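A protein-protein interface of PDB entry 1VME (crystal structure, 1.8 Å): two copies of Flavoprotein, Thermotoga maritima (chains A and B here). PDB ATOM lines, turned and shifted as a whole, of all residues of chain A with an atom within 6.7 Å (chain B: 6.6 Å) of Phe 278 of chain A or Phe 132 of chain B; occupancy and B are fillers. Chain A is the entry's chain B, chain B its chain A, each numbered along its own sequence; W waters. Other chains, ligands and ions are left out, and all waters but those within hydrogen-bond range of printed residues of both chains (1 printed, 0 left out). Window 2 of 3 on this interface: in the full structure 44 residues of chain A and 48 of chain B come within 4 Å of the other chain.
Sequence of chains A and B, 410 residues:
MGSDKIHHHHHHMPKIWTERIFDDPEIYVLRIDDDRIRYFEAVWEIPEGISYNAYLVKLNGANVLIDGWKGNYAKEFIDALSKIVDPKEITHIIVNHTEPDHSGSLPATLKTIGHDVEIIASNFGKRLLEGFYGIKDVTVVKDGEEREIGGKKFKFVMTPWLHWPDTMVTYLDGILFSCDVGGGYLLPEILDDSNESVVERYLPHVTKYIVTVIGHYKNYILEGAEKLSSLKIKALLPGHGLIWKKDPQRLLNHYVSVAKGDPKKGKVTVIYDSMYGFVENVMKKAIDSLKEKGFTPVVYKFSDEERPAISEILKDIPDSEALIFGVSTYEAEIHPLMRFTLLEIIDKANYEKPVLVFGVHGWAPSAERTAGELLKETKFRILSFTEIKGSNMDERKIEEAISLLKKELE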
ATOM      1  N   SER A 274       7.543 -30.277 -23.969  1.00  0.00           N
ATOM      2  CA  SER A 274       7.555 -28.887 -23.534  1.00  0.00           C
ATOM      3  C   SER A 274       6.185 -28.352 -23.784  1.00  0.00           C
ATOM      4  O   SER A 274       5.772 -28.197 -24.916  1.00  0.00           O
ATOM      5  CB  SER A 274       8.607 -28.016 -24.232  1.00  0.00           C
ATOM      6  OG  SER A 274       8.650 -26.700 -23.621  1.00  0.00           O
ATOM      7  N   MET A 275       5.501 -28.074 -22.700  1.00  0.00           N
ATOM      8  CA  MET A 275       4.146 -27.527 -22.793  1.00  0.00           C
ATOM      9  C   MET A 275       4.148 -26.038 -23.007  1.00  0.00           C
ATOM     10  O   MET A 275       3.464 -25.524 -23.889  1.00  0.00           O
ATOM     11  CB  MET A 275       3.423 -27.885 -21.542  1.00  0.00           C
ATOM     12  CG  MET A 275       3.376 -29.408 -21.351  1.00  0.00           C
ATOM     13  SD  MET A 275       2.197 -29.941 -19.897  1.00  0.00           S
ATOM     14  CE  MET A 275       0.961 -28.520 -20.499  1.00  0.00           C
ATOM     15  N   TYR A 276       4.935 -25.317 -22.231  1.00  0.00           N
ATOM     16  CA  TYR A 276       4.936 -23.867 -22.317  1.00  0.00           C
ATOM     17  C   TYR A 276       6.273 -23.202 -22.460  1.00  0.00           C
ATOM     18  O   TYR A 276       6.406 -22.003 -22.259  1.00  0.00           O
ATOM     19  CB  TYR A 276       4.232 -23.363 -21.070  1.00  0.00           C
ATOM     20  CG  TYR A 276       2.793 -23.712 -21.124  1.00  0.00           C
ATOM     21  CD1 TYR A 276       1.976 -23.157 -22.137  1.00  0.00           C
ATOM     22  CD2 TYR A 276       2.231 -24.588 -20.211  1.00  0.00           C
ATOM     23  CE1 TYR A 276       0.617 -23.452 -22.235  1.00  0.00           C
ATOM     24  CE2 TYR A 276       0.895 -24.904 -20.279  1.00  0.00           C
ATOM     25  CZ  TYR A 276       0.045 -24.333 -21.310  1.00  0.00           C
ATOM     26  OH  TYR A 276      -1.359 -24.588 -21.459  1.00  0.00           O
ATOM     27  N   GLY A 277       7.296 -23.982 -22.774  1.00  0.00           N
ATOM     28  CA  GLY A 277       8.580 -23.393 -23.064  1.00  0.00           C
ATOM     29  C   GLY A 277       9.620 -23.478 -21.979  1.00  0.00           C
ATOM     30  O   GLY A 277      10.787 -23.206 -22.235  1.00  0.00           O
ATOM     31  N   PHE A 278       9.222 -23.877 -20.772  1.00  0.00           N
ATOM     32  CA  PHE A 278      10.159 -23.990 -19.671  1.00  0.00           C
ATOM     33  C   PHE A 278      11.132 -25.175 -19.860  1.00  0.00           C
ATOM     34  O   PHE A 278      12.321 -25.041 -19.645  1.00  0.00           O
ATOM     35  CB  PHE A 278       9.432 -24.094 -18.346  1.00  0.00           C
ATOM     36  CG  PHE A 278       8.632 -22.874 -18.014  1.00  0.00           C
ATOM     37  CD1 PHE A 278       9.255 -21.747 -17.531  1.00  0.00           C
ATOM     38  CD2 PHE A 278       7.272 -22.830 -18.257  1.00  0.00           C
ATOM     39  CE1 PHE A 278       8.535 -20.617 -17.247  1.00  0.00           C
ATOM     40  CE2 PHE A 278       6.552 -21.699 -17.970  1.00  0.00           C
ATOM     41  CZ  PHE A 278       7.177 -20.597 -17.463  1.00  0.00           C
ATOM     42  N   VAL A 279      10.611 -26.348 -20.203  1.00  0.00           N
ATOM     43  CA  VAL A 279      11.454 -27.472 -20.519  1.00  0.00           C
ATOM     44  C   VAL A 279      12.304 -27.162 -21.759  1.00  0.00           C
ATOM     45  O   VAL A 279      13.511 -27.447 -21.789  1.00  0.00           O
ATOM     46  CB  VAL A 279      10.650 -28.752 -20.732  1.00  0.00           C
ATOM     47  CG1 VAL A 279      11.584 -29.901 -21.091  1.00  0.00           C
ATOM     48  CG2 VAL A 279       9.852 -29.096 -19.479  1.00  0.00           C
ATOM     49  N   GLU A 280      11.685 -26.554 -22.772  1.00  0.00           N
ATOM     50  CA  GLU A 280      12.426 -26.168 -24.012  1.00  0.00           C
ATOM     51  C   GLU A 280      13.647 -25.298 -23.706  1.00  0.00           C
ATOM     52  O   GLU A 280      14.729 -25.501 -24.245  1.00  0.00           O
ATOM     53  CB  GLU A 280      11.494 -25.458 -24.993  1.00  0.00           C
ATOM     54  CG  GLU A 280      12.178 -24.793 -26.194  1.00  0.00           C
ATOM     55  CD  GLU A 280      12.932 -25.765 -27.065  1.00  0.00           C
ATOM     56  OE1 GLU A 280      12.579 -26.959 -27.029  1.00  0.00           O
ATOM     57  OE2 GLU A 280      13.886 -25.335 -27.795  1.00  0.00           O
ATOM     58  N   ASN A 281      13.482 -24.337 -22.812  1.00  0.00           N
ATOM     59  CA  ASN A 281      14.577 -23.446 -22.448  1.00  0.00           C
ATOM     60  C   ASN A 281      15.785 -24.147 -21.823  1.00  0.00           C
ATOM     61  O   ASN A 281      16.945 -23.842 -22.149  1.00  0.00           O
ATOM     62  CB  ASN A 281      14.051 -22.326 -21.550  1.00  0.00           C
ATOM     63  CG  ASN A 281      14.987 -21.161 -21.495  1.00  0.00           C
ATOM     64  OD1 ASN A 281      15.967 -21.184 -20.756  1.00  0.00           O
ATOM     65  ND2 ASN A 281      14.714 -20.141 -22.298  1.00  0.00           N
ATOM     66  N   VAL A 282      15.517 -25.096 -20.942  1.00  0.00           N
ATOM     67  CA  VAL A 282      16.534 -25.908 -20.332  1.00  0.00           C
ATOM     68  C   VAL A 282      17.181 -26.853 -21.345  1.00  0.00           C
ATOM     69  O   VAL A 282      18.443 -27.020 -21.358  1.00  0.00           O
ATOM     70  CB  VAL A 282      15.944 -26.661 -19.146  1.00  0.00           C
ATOM     71  CG1 VAL A 282      16.871 -27.749 -18.618  1.00  0.00           C
ATOM     72  CG2 VAL A 282      15.573 -25.645 -18.041  1.00  0.00           C
ATOM     73  N   MET A 283      16.350 -27.504 -22.178  1.00  0.00           N
ATOM     74  CA  MET A 283      16.867 -28.458 -23.182  1.00  0.00           C
ATOM     75  C   MET A 283      17.747 -27.752 -24.219  1.00  0.00           C
ATOM     76  O   MET A 283      18.753 -28.315 -24.635  1.00  0.00           O
ATOM     77  CB  MET A 283      15.740 -29.206 -23.904  1.00  0.00           C
ATOM     78  CG  MET A 283      14.900 -30.104 -23.078  1.00  0.00           C
ATOM     79  SD  MET A 283      15.995 -31.669 -22.436  1.00  0.00           S
ATOM     80  CE  MET A 283      15.974 -30.907 -20.823  1.00  0.00           C
ATOM     81  N   VAL A 360      10.565 -30.924 -14.363  1.00  0.00           N
ATOM     82  CA  VAL A 360       9.861 -29.897 -13.608  1.00  0.00           C
ATOM     83  C   VAL A 360       9.349 -30.483 -12.289  1.00  0.00           C
ATOM     84  O   VAL A 360       8.822 -31.600 -12.260  1.00  0.00           O
ATOM     85  CB  VAL A 360       8.666 -29.355 -14.385  1.00  0.00           C
ATOM     86  CG1 VAL A 360       7.908 -28.358 -13.529  1.00  0.00           C
ATOM     87  CG2 VAL A 360       9.192 -28.680 -15.683  1.00  0.00           C
ATOM     88  N   TRP A 363       3.267 -30.519  -8.386  1.00  0.00           N
ATOM     89  CA  TRP A 363       2.534 -30.643  -7.138  1.00  0.00           C
ATOM     90  C   TRP A 363       1.700 -31.910  -7.313  1.00  0.00           C
ATOM     91  O   TRP A 363       0.644 -32.036  -6.717  1.00  0.00           O
ATOM     92  CB  TRP A 363       1.640 -29.412  -6.869  1.00  0.00           C
ATOM     93  CG  TRP A 363       0.688 -29.155  -7.995  1.00  0.00           C
ATOM     94  CD1 TRP A 363      -0.449 -29.803  -8.248  1.00  0.00           C
ATOM     95  CD2 TRP A 363       0.899 -28.259  -9.077  1.00  0.00           C
ATOM     96  NE1 TRP A 363      -1.009 -29.356  -9.423  1.00  0.00           N
ATOM     97  CE2 TRP A 363      -0.200 -28.392  -9.947  1.00  0.00           C
ATOM     98  CE3 TRP A 363       1.928 -27.359  -9.410  1.00  0.00           C
ATOM     99  CZ2 TRP A 363      -0.330 -27.646 -11.100  1.00  0.00           C
ATOM    100  CZ3 TRP A 363       1.811 -26.617 -10.572  1.00  0.00           C
ATOM    101  CH2 TRP A 363       0.678 -26.760 -11.400  1.00  0.00           C
ATOM    102  N   ILE A 388      14.013 -28.487 -13.344  1.00  0.00           N
ATOM    103  CA  ILE A 388      13.734 -27.389 -14.247  1.00  0.00           C
ATOM    104  C   ILE A 388      12.865 -26.376 -13.495  1.00  0.00           C
ATOM    105  O   ILE A 388      11.808 -26.737 -12.977  1.00  0.00           O
ATOM    106  CB  ILE A 388      13.005 -27.894 -15.521  1.00  0.00           C
ATOM    107  CG1 ILE A 388      13.939 -28.788 -16.340  1.00  0.00           C
ATOM    108  CG2 ILE A 388      12.468 -26.701 -16.368  1.00  0.00           C
ATOM    109  CD1 ILE A 388      13.234 -29.594 -17.422  1.00  0.00           C
ATOM    110  N   LYS A 389      13.327 -25.127 -13.436  1.00  0.00           N
ATOM    111  CA  LYS A 389      12.600 -24.033 -12.792  1.00  0.00           C
ATOM    112  C   LYS A 389      12.414 -22.884 -13.781  1.00  0.00           C
ATOM    113  O   LYS A 389      13.219 -22.718 -14.691  1.00  0.00           O
ATOM    114  CB  LYS A 389      13.382 -23.531 -11.569  1.00  0.00           C
ATOM    115  CG  LYS A 389      13.783 -24.635 -10.601  1.00  0.00           C
ATOM    116  CD  LYS A 389      14.361 -24.056  -9.328  1.00  0.00           C
ATOM    117  CE  LYS A 389      14.500 -25.112  -8.252  1.00  0.00           C
ATOM    118  NZ  LYS A 389      15.267 -24.587  -7.066  1.00  0.00           N
ATOM    119  N   GLY A 390      11.371 -22.081 -13.607  1.00  0.00           N
ATOM    120  CA  GLY A 390      11.063 -21.025 -14.577  1.00  0.00           C
ATOM    121  C   GLY A 390      11.661 -19.673 -14.240  1.00  0.00           C
ATOM    122  O   GLY A 390      11.747 -18.783 -15.095  1.00  0.00           O
ATOM    123  N   SER A 391      12.025 -19.502 -12.977  1.00  0.00           N
ATOM    124  CA  SER A 391      12.640 -18.289 -12.508  1.00  0.00           C
ATOM    125  C   SER A 391      13.757 -18.667 -11.537  1.00  0.00           C
ATOM    126  O   SER A 391      13.680 -19.697 -10.872  1.00  0.00           O
ATOM    127  CB  SER A 391      11.585 -17.413 -11.823  1.00  0.00           C
ATOM    128  OG  SER A 391      11.967 -16.056 -11.900  1.00  0.00           O
ATOM    129  N   THR B  98      -3.065 -19.368 -13.292  1.00  0.00           N
ATOM    130  CA  THR B  98      -1.710 -18.948 -13.660  1.00  0.00           C
ATOM    131  C   THR B  98      -1.071 -19.735 -14.786  1.00  0.00           C
ATOM    132  O   THR B  98       0.079 -19.491 -15.147  1.00  0.00           O
ATOM    133  CB  THR B  98      -0.752 -19.018 -12.460  1.00  0.00           C
ATOM    134  OG1 THR B  98      -0.560 -20.375 -12.053  1.00  0.00           O
ATOM    135  CG2 THR B  98      -1.248 -18.206 -11.297  1.00  0.00           C
ATOM    136  N   GLU B  99      -1.781 -20.677 -15.375  1.00  0.00           N
ATOM    137  CA  GLU B  99      -1.197 -21.492 -16.416  1.00  0.00           C
ATOM    138  C   GLU B  99      -0.780 -20.590 -17.583  1.00  0.00           C
ATOM    139  O   GLU B  99      -1.471 -19.627 -17.909  1.00  0.00           O
ATOM    140  CB  GLU B  99      -2.158 -22.587 -16.868  1.00  0.00           C
ATOM    141  CG  GLU B  99      -1.543 -23.604 -17.797  1.00  0.00           C
ATOM    142  CD  GLU B  99      -2.481 -24.778 -18.102  1.00  0.00           C
ATOM    143  OE1 GLU B  99      -3.474 -24.905 -17.389  1.00  0.00           O
ATOM    144  OE2 GLU B  99      -2.195 -25.587 -19.016  1.00  0.00           O
ATOM    145  N   PRO B 100       0.372 -20.887 -18.189  1.00  0.00           N
ATOM    146  CA  PRO B 100       0.872 -19.969 -19.217  1.00  0.00           C
ATOM    147  C   PRO B 100       0.075 -19.722 -20.458  1.00  0.00           C
ATOM    148  O   PRO B 100       0.400 -18.750 -21.178  1.00  0.00           O
ATOM    149  CB  PRO B 100       2.287 -20.519 -19.519  1.00  0.00           C
ATOM    150  CG  PRO B 100       2.659 -21.203 -18.240  1.00  0.00           C
ATOM    151  CD  PRO B 100       1.406 -21.873 -17.818  1.00  0.00           C
ATOM    152  N   SER B 103      -1.301 -16.670 -18.639  1.00  0.00           N
ATOM    153  CA  SER B 103      -0.383 -15.771 -17.981  1.00  0.00           C
ATOM    154  C   SER B 103       0.911 -15.482 -18.729  1.00  0.00           C
ATOM    155  O   SER B 103       1.707 -14.681 -18.256  1.00  0.00           O
ATOM    156  CB  SER B 103      -0.011 -16.350 -16.618  1.00  0.00           C
ATOM    157  OG  SER B 103       0.816 -17.512 -16.757  1.00  0.00           O
ATOM    158  N   ARG B 127       2.071 -18.352  -5.448  1.00  0.00           N
ATOM    159  CA  ARG B 127       3.260 -19.212  -5.456  1.00  0.00           C
ATOM    160  C   ARG B 127       3.720 -19.553  -6.871  1.00  0.00           C
ATOM    161  O   ARG B 127       4.922 -19.609  -7.141  1.00  0.00           O
ATOM    162  CB  ARG B 127       2.982 -20.499  -4.667  1.00  0.00           C
ATOM    163  CG  ARG B 127       2.754 -20.199  -3.172  1.00  0.00           C
ATOM    164  CD  ARG B 127       2.063 -21.332  -2.428  1.00  0.00           C
ATOM    165  NE  ARG B 127       2.842 -22.562  -2.467  1.00  0.00           N
ATOM    166  CZ  ARG B 127       2.449 -23.705  -1.910  1.00  0.00           C
ATOM    167  NH1 ARG B 127       1.283 -23.775  -1.260  1.00  0.00           N
ATOM    168  NH2 ARG B 127       3.224 -24.784  -2.002  1.00  0.00           N
ATOM    169  N   LEU B 128       2.764 -19.797  -7.749  1.00  0.00           N
ATOM    170  CA  LEU B 128       3.056 -20.190  -9.130  1.00  0.00           C
ATOM    171  C   LEU B 128       3.572 -18.999  -9.914  1.00  0.00           C
ATOM    172  O   LEU B 128       4.453 -19.153 -10.758  1.00  0.00           O
ATOM    173  CB  LEU B 128       1.841 -20.798  -9.802  1.00  0.00           C
ATOM    174  CG  LEU B 128       1.437 -22.169  -9.250  1.00  0.00           C
ATOM    175  CD1 LEU B 128       0.088 -22.593  -9.805  1.00  0.00           C
ATOM    176  CD2 LEU B 128       2.509 -23.248  -9.503  1.00  0.00           C
ATOM    177  N   LEU B 129       3.050 -17.805  -9.656  1.00  0.00           N
ATOM    178  CA  LEU B 129       3.570 -16.626 -10.375  1.00  0.00           C
ATOM    179  C   LEU B 129       5.025 -16.342 -10.006  1.00  0.00           C
ATOM    180  O   LEU B 129       5.810 -15.869 -10.842  1.00  0.00           O
ATOM    181  CB  LEU B 129       2.747 -15.382 -10.099  1.00  0.00           C
ATOM    182  CG  LEU B 129       1.344 -15.421 -10.701  1.00  0.00           C
ATOM    183  CD1 LEU B 129       0.492 -14.351 -10.168  1.00  0.00           C
ATOM    184  CD2 LEU B 129       1.445 -15.374 -12.209  1.00  0.00           C
ATOM    185  N   GLU B 130       5.366 -16.601  -8.753  1.00  0.00           N
ATOM    186  CA  GLU B 130       6.757 -16.479  -8.312  1.00  0.00           C
ATOM    187  C   GLU B 130       7.598 -17.548  -9.000  1.00  0.00           C
ATOM    188  O   GLU B 130       8.681 -17.274  -9.495  1.00  0.00           O
ATOM    189  CB  GLU B 130       6.859 -16.605  -6.799  1.00  0.00           C
ATOM    190  CG  GLU B 130       8.297 -16.439  -6.253  1.00  0.00           C
ATOM    191  N   GLY B 131       7.078 -18.764  -9.060  1.00  0.00           N
ATOM    192  CA  GLY B 131       7.793 -19.874  -9.662  1.00  0.00           C
ATOM    193  C   GLY B 131       8.047 -19.710 -11.149  1.00  0.00           C
ATOM    194  O   GLY B 131       9.165 -19.936 -11.633  1.00  0.00           O
ATOM    195  N   PHE B 132       7.015 -19.312 -11.864  1.00  0.00           N
ATOM    196  CA  PHE B 132       7.085 -19.183 -13.319  1.00  0.00           C
ATOM    197  C   PHE B 132       7.897 -17.957 -13.768  1.00  0.00           C
ATOM    198  O   PHE B 132       8.695 -18.057 -14.708  1.00  0.00           O
ATOM    199  CB  PHE B 132       5.705 -19.047 -13.920  1.00  0.00           C
ATOM    200  CG  PHE B 132       4.856 -20.320 -13.858  1.00  0.00           C
ATOM    201  CD1 PHE B 132       5.428 -21.574 -13.880  1.00  0.00           C
ATOM    202  CD2 PHE B 132       3.487 -20.229 -13.837  1.00  0.00           C
ATOM    203  CE1 PHE B 132       4.635 -22.718 -13.818  1.00  0.00           C
ATOM    204  CE2 PHE B 132       2.680 -21.367 -13.790  1.00  0.00           C
ATOM    205  CZ  PHE B 132       3.256 -22.604 -13.782  1.00  0.00           C
ATOM    206  N   TYR B 133       7.645 -16.822 -13.115  1.00  0.00           N
ATOM    207  CA  TYR B 133       8.058 -15.518 -13.617  1.00  0.00           C
ATOM    208  C   TYR B 133       8.852 -14.656 -12.648  1.00  0.00           C
ATOM    209  O   TYR B 133       9.331 -13.580 -13.041  1.00  0.00           O
ATOM    210  CB  TYR B 133       6.835 -14.728 -14.052  1.00  0.00           C
ATOM    211  CG  TYR B 133       5.901 -15.462 -14.976  1.00  0.00           C
ATOM    212  CD1 TYR B 133       6.347 -15.933 -16.199  1.00  0.00           C
ATOM    213  CD2 TYR B 133       4.571 -15.656 -14.644  1.00  0.00           C
ATOM    214  CE1 TYR B 133       5.498 -16.612 -17.055  1.00  0.00           C
ATOM    215  CE2 TYR B 133       3.684 -16.347 -15.506  1.00  0.00           C
ATOM    216  CZ  TYR B 133       4.170 -16.819 -16.709  1.00  0.00           C
ATOM    217  OH  TYR B 133       3.375 -17.493 -17.596  1.00  0.00           O
ATOM    218  N   GLY B 134       9.028 -15.113 -11.409  1.00  0.00           N
ATOM    219  CA  GLY B 134       9.676 -14.301 -10.381  1.00  0.00           C
ATOM    220  C   GLY B 134       8.914 -13.054  -9.937  1.00  0.00           C
ATOM    221  O   GLY B 134       9.503 -12.141  -9.351  1.00  0.00           O
ATOM    222  N   ILE B 135       7.610 -13.047 -10.167  1.00  0.00           N
ATOM    223  CA  ILE B 135       6.701 -11.969  -9.731  1.00  0.00           C
ATOM    224  C   ILE B 135       6.455 -12.153  -8.256  1.00  0.00           C
ATOM    225  O   ILE B 135       6.013 -13.217  -7.846  1.00  0.00           O
ATOM    226  CB  ILE B 135       5.393 -12.004 -10.530  1.00  0.00           C
ATOM    227  CG1 ILE B 135       5.673 -11.633 -11.981  1.00  0.00           C
ATOM    228  CG2 ILE B 135       4.367 -11.008  -9.962  1.00  0.00           C
ATOM    229  CD1 ILE B 135       4.563 -12.024 -12.942  1.00  0.00           C
ATOM    230  N   TRP B 164      -6.325 -26.787 -11.849  1.00  0.00           N
ATOM    231  CA  TRP B 164      -5.173 -26.644 -10.954  1.00  0.00           C
ATOM    232  C   TRP B 164      -5.652 -26.166  -9.591  1.00  0.00           C
ATOM    233  O   TRP B 164      -6.734 -25.616  -9.468  1.00  0.00           O
ATOM    234  CB  TRP B 164      -4.202 -25.603 -11.532  1.00  0.00           C
ATOM    235  CG  TRP B 164      -3.245 -26.094 -12.590  1.00  0.00           C
ATOM    236  CD1 TRP B 164      -3.252 -27.292 -13.252  1.00  0.00           C
ATOM    237  CD2 TRP B 164      -2.161 -25.341 -13.136  1.00  0.00           C
ATOM    238  NE1 TRP B 164      -2.206 -27.339 -14.159  1.00  0.00           N
ATOM    239  CE2 TRP B 164      -1.536 -26.144 -14.121  1.00  0.00           C
ATOM    240  CE3 TRP B 164      -1.673 -24.056 -12.899  1.00  0.00           C
ATOM    241  CZ2 TRP B 164      -0.411 -25.708 -14.836  1.00  0.00           C
ATOM    242  CZ3 TRP B 164      -0.546 -23.632 -13.604  1.00  0.00           C
ATOM    243  CH2 TRP B 164       0.077 -24.464 -14.537  1.00  0.00           C
ATOM    244  N   ASP B 166      -4.831 -23.573  -8.107  1.00  0.00           N
ATOM    245  CA  ASP B 166      -4.841 -22.109  -8.048  1.00  0.00           C
ATOM    246  C   ASP B 166      -6.135 -21.467  -8.530  1.00  0.00           C
ATOM    247  O   ASP B 166      -6.315 -20.259  -8.443  1.00  0.00           O
ATOM    248  CB  ASP B 166      -3.642 -21.491  -8.812  1.00  0.00           C
ATOM    249  CG  ASP B 166      -3.757 -21.604 -10.320  1.00  0.00           C
ATOM    250  OD1 ASP B 166      -4.608 -22.362 -10.834  1.00  0.00           O
ATOM    251  OD2 ASP B 166      -3.007 -20.888 -11.023  1.00  0.00           O
HETATM  252  O   HOH W   1       9.859 -17.030 -16.938  1.00  0.00           O
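N of Gly 134 of chain B sits at hydrogen-bond distance from OG of Ser 391 of chain A, 3.1 Å away.
The backbone carbonyl oxygen of Gly 390 of chain A lies close to the backbone carbonyl oxygen of Phe 132 of chain B, at 3.2 Å.
OE2 of Glu 99 of chain B lies within hydrogen-bond range of OH of Tyr 276 of chain A (2.8 Å).
The backbone NH (N) of Ser 391 of chain A sits at hydrogen-bond distance from the backbone carbonyl oxygen (O) of Gly 131 of chain B.
The backbone carbonyl oxygen of Leu 129 of chain B is in hydrogen-bond range of the backbone NH of Gly 134 of chain B, at 3.4 Å.
The side-chain hydroxyl of Ser 103 of chain B lies within hydrogen-bond range of the side-chain hydroxyl of Tyr 133 of chain B, at 2.7 Å.
OG of Ser 103 of chain B sits at hydrogen-bond distance from O of Glu 99 of chain B (3.3 Å).
Among the printed residues, pairs that only touch across the chains: Tyr 276 of chain A with Pro 100 of chain B (3.6 Å), Phe 278 of chain A with Pro 100 of chain B (3.9 Å), Phe 278 of chain A with Phe 132 of chain B (3.6 Å), Trp 363 of chain A with Leu 128 of chain B (3.6 Å), Trp 363 of chain A with Trp 164 of chain B (3.6 Å), Gly 390 of chain A with Gly 131 of chain B (3.6 Å), Ser 391 of chain A with Glu 130 of chain B (3.7 Å) and Ser 391 of chain A with Tyr 133 of chain B (3.5 Å).
Of the printed residues of chain B, Tyr 276 of chain A touches Glu 99 (2.8 Å) and Pro 100 (3.6 Å).
Printed residues of chain B within 4 Å of Phe 278 of chain A: Pro 100 (3.9 Å) and Phe 132 (3.6 Å).
Val 279 of chain A touches none of the printed residues of chain B.
Lys 389 of chain A touches none of the printed residues of chain B.
Printed residues of chain A within 4 Å of Leu 128 of chain B: Trp 363 (3.6 Å).
Of the printed residues of chain A, Phe 132 of chain B touches Phe 278 and Gly 390.
Of the printed residues of chain A, Tyr 133 of chain B touches Ser 391 (3.5 Å).
The nearest printed residue of chain A that does not touch Gly 131 of chain B is Lys 389 of chain A (4.9 Å).
Of the 16 printed residues of chain A, 5 touch a printed residue of chain B.
Among the printed residues, 12 pairs touch across the chains.
No position is printed for both chains.
Water W1 bridges O of Phe 132 of chain B (2.7 Å) and O of Gly 390 of chain A (3.2 Å).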
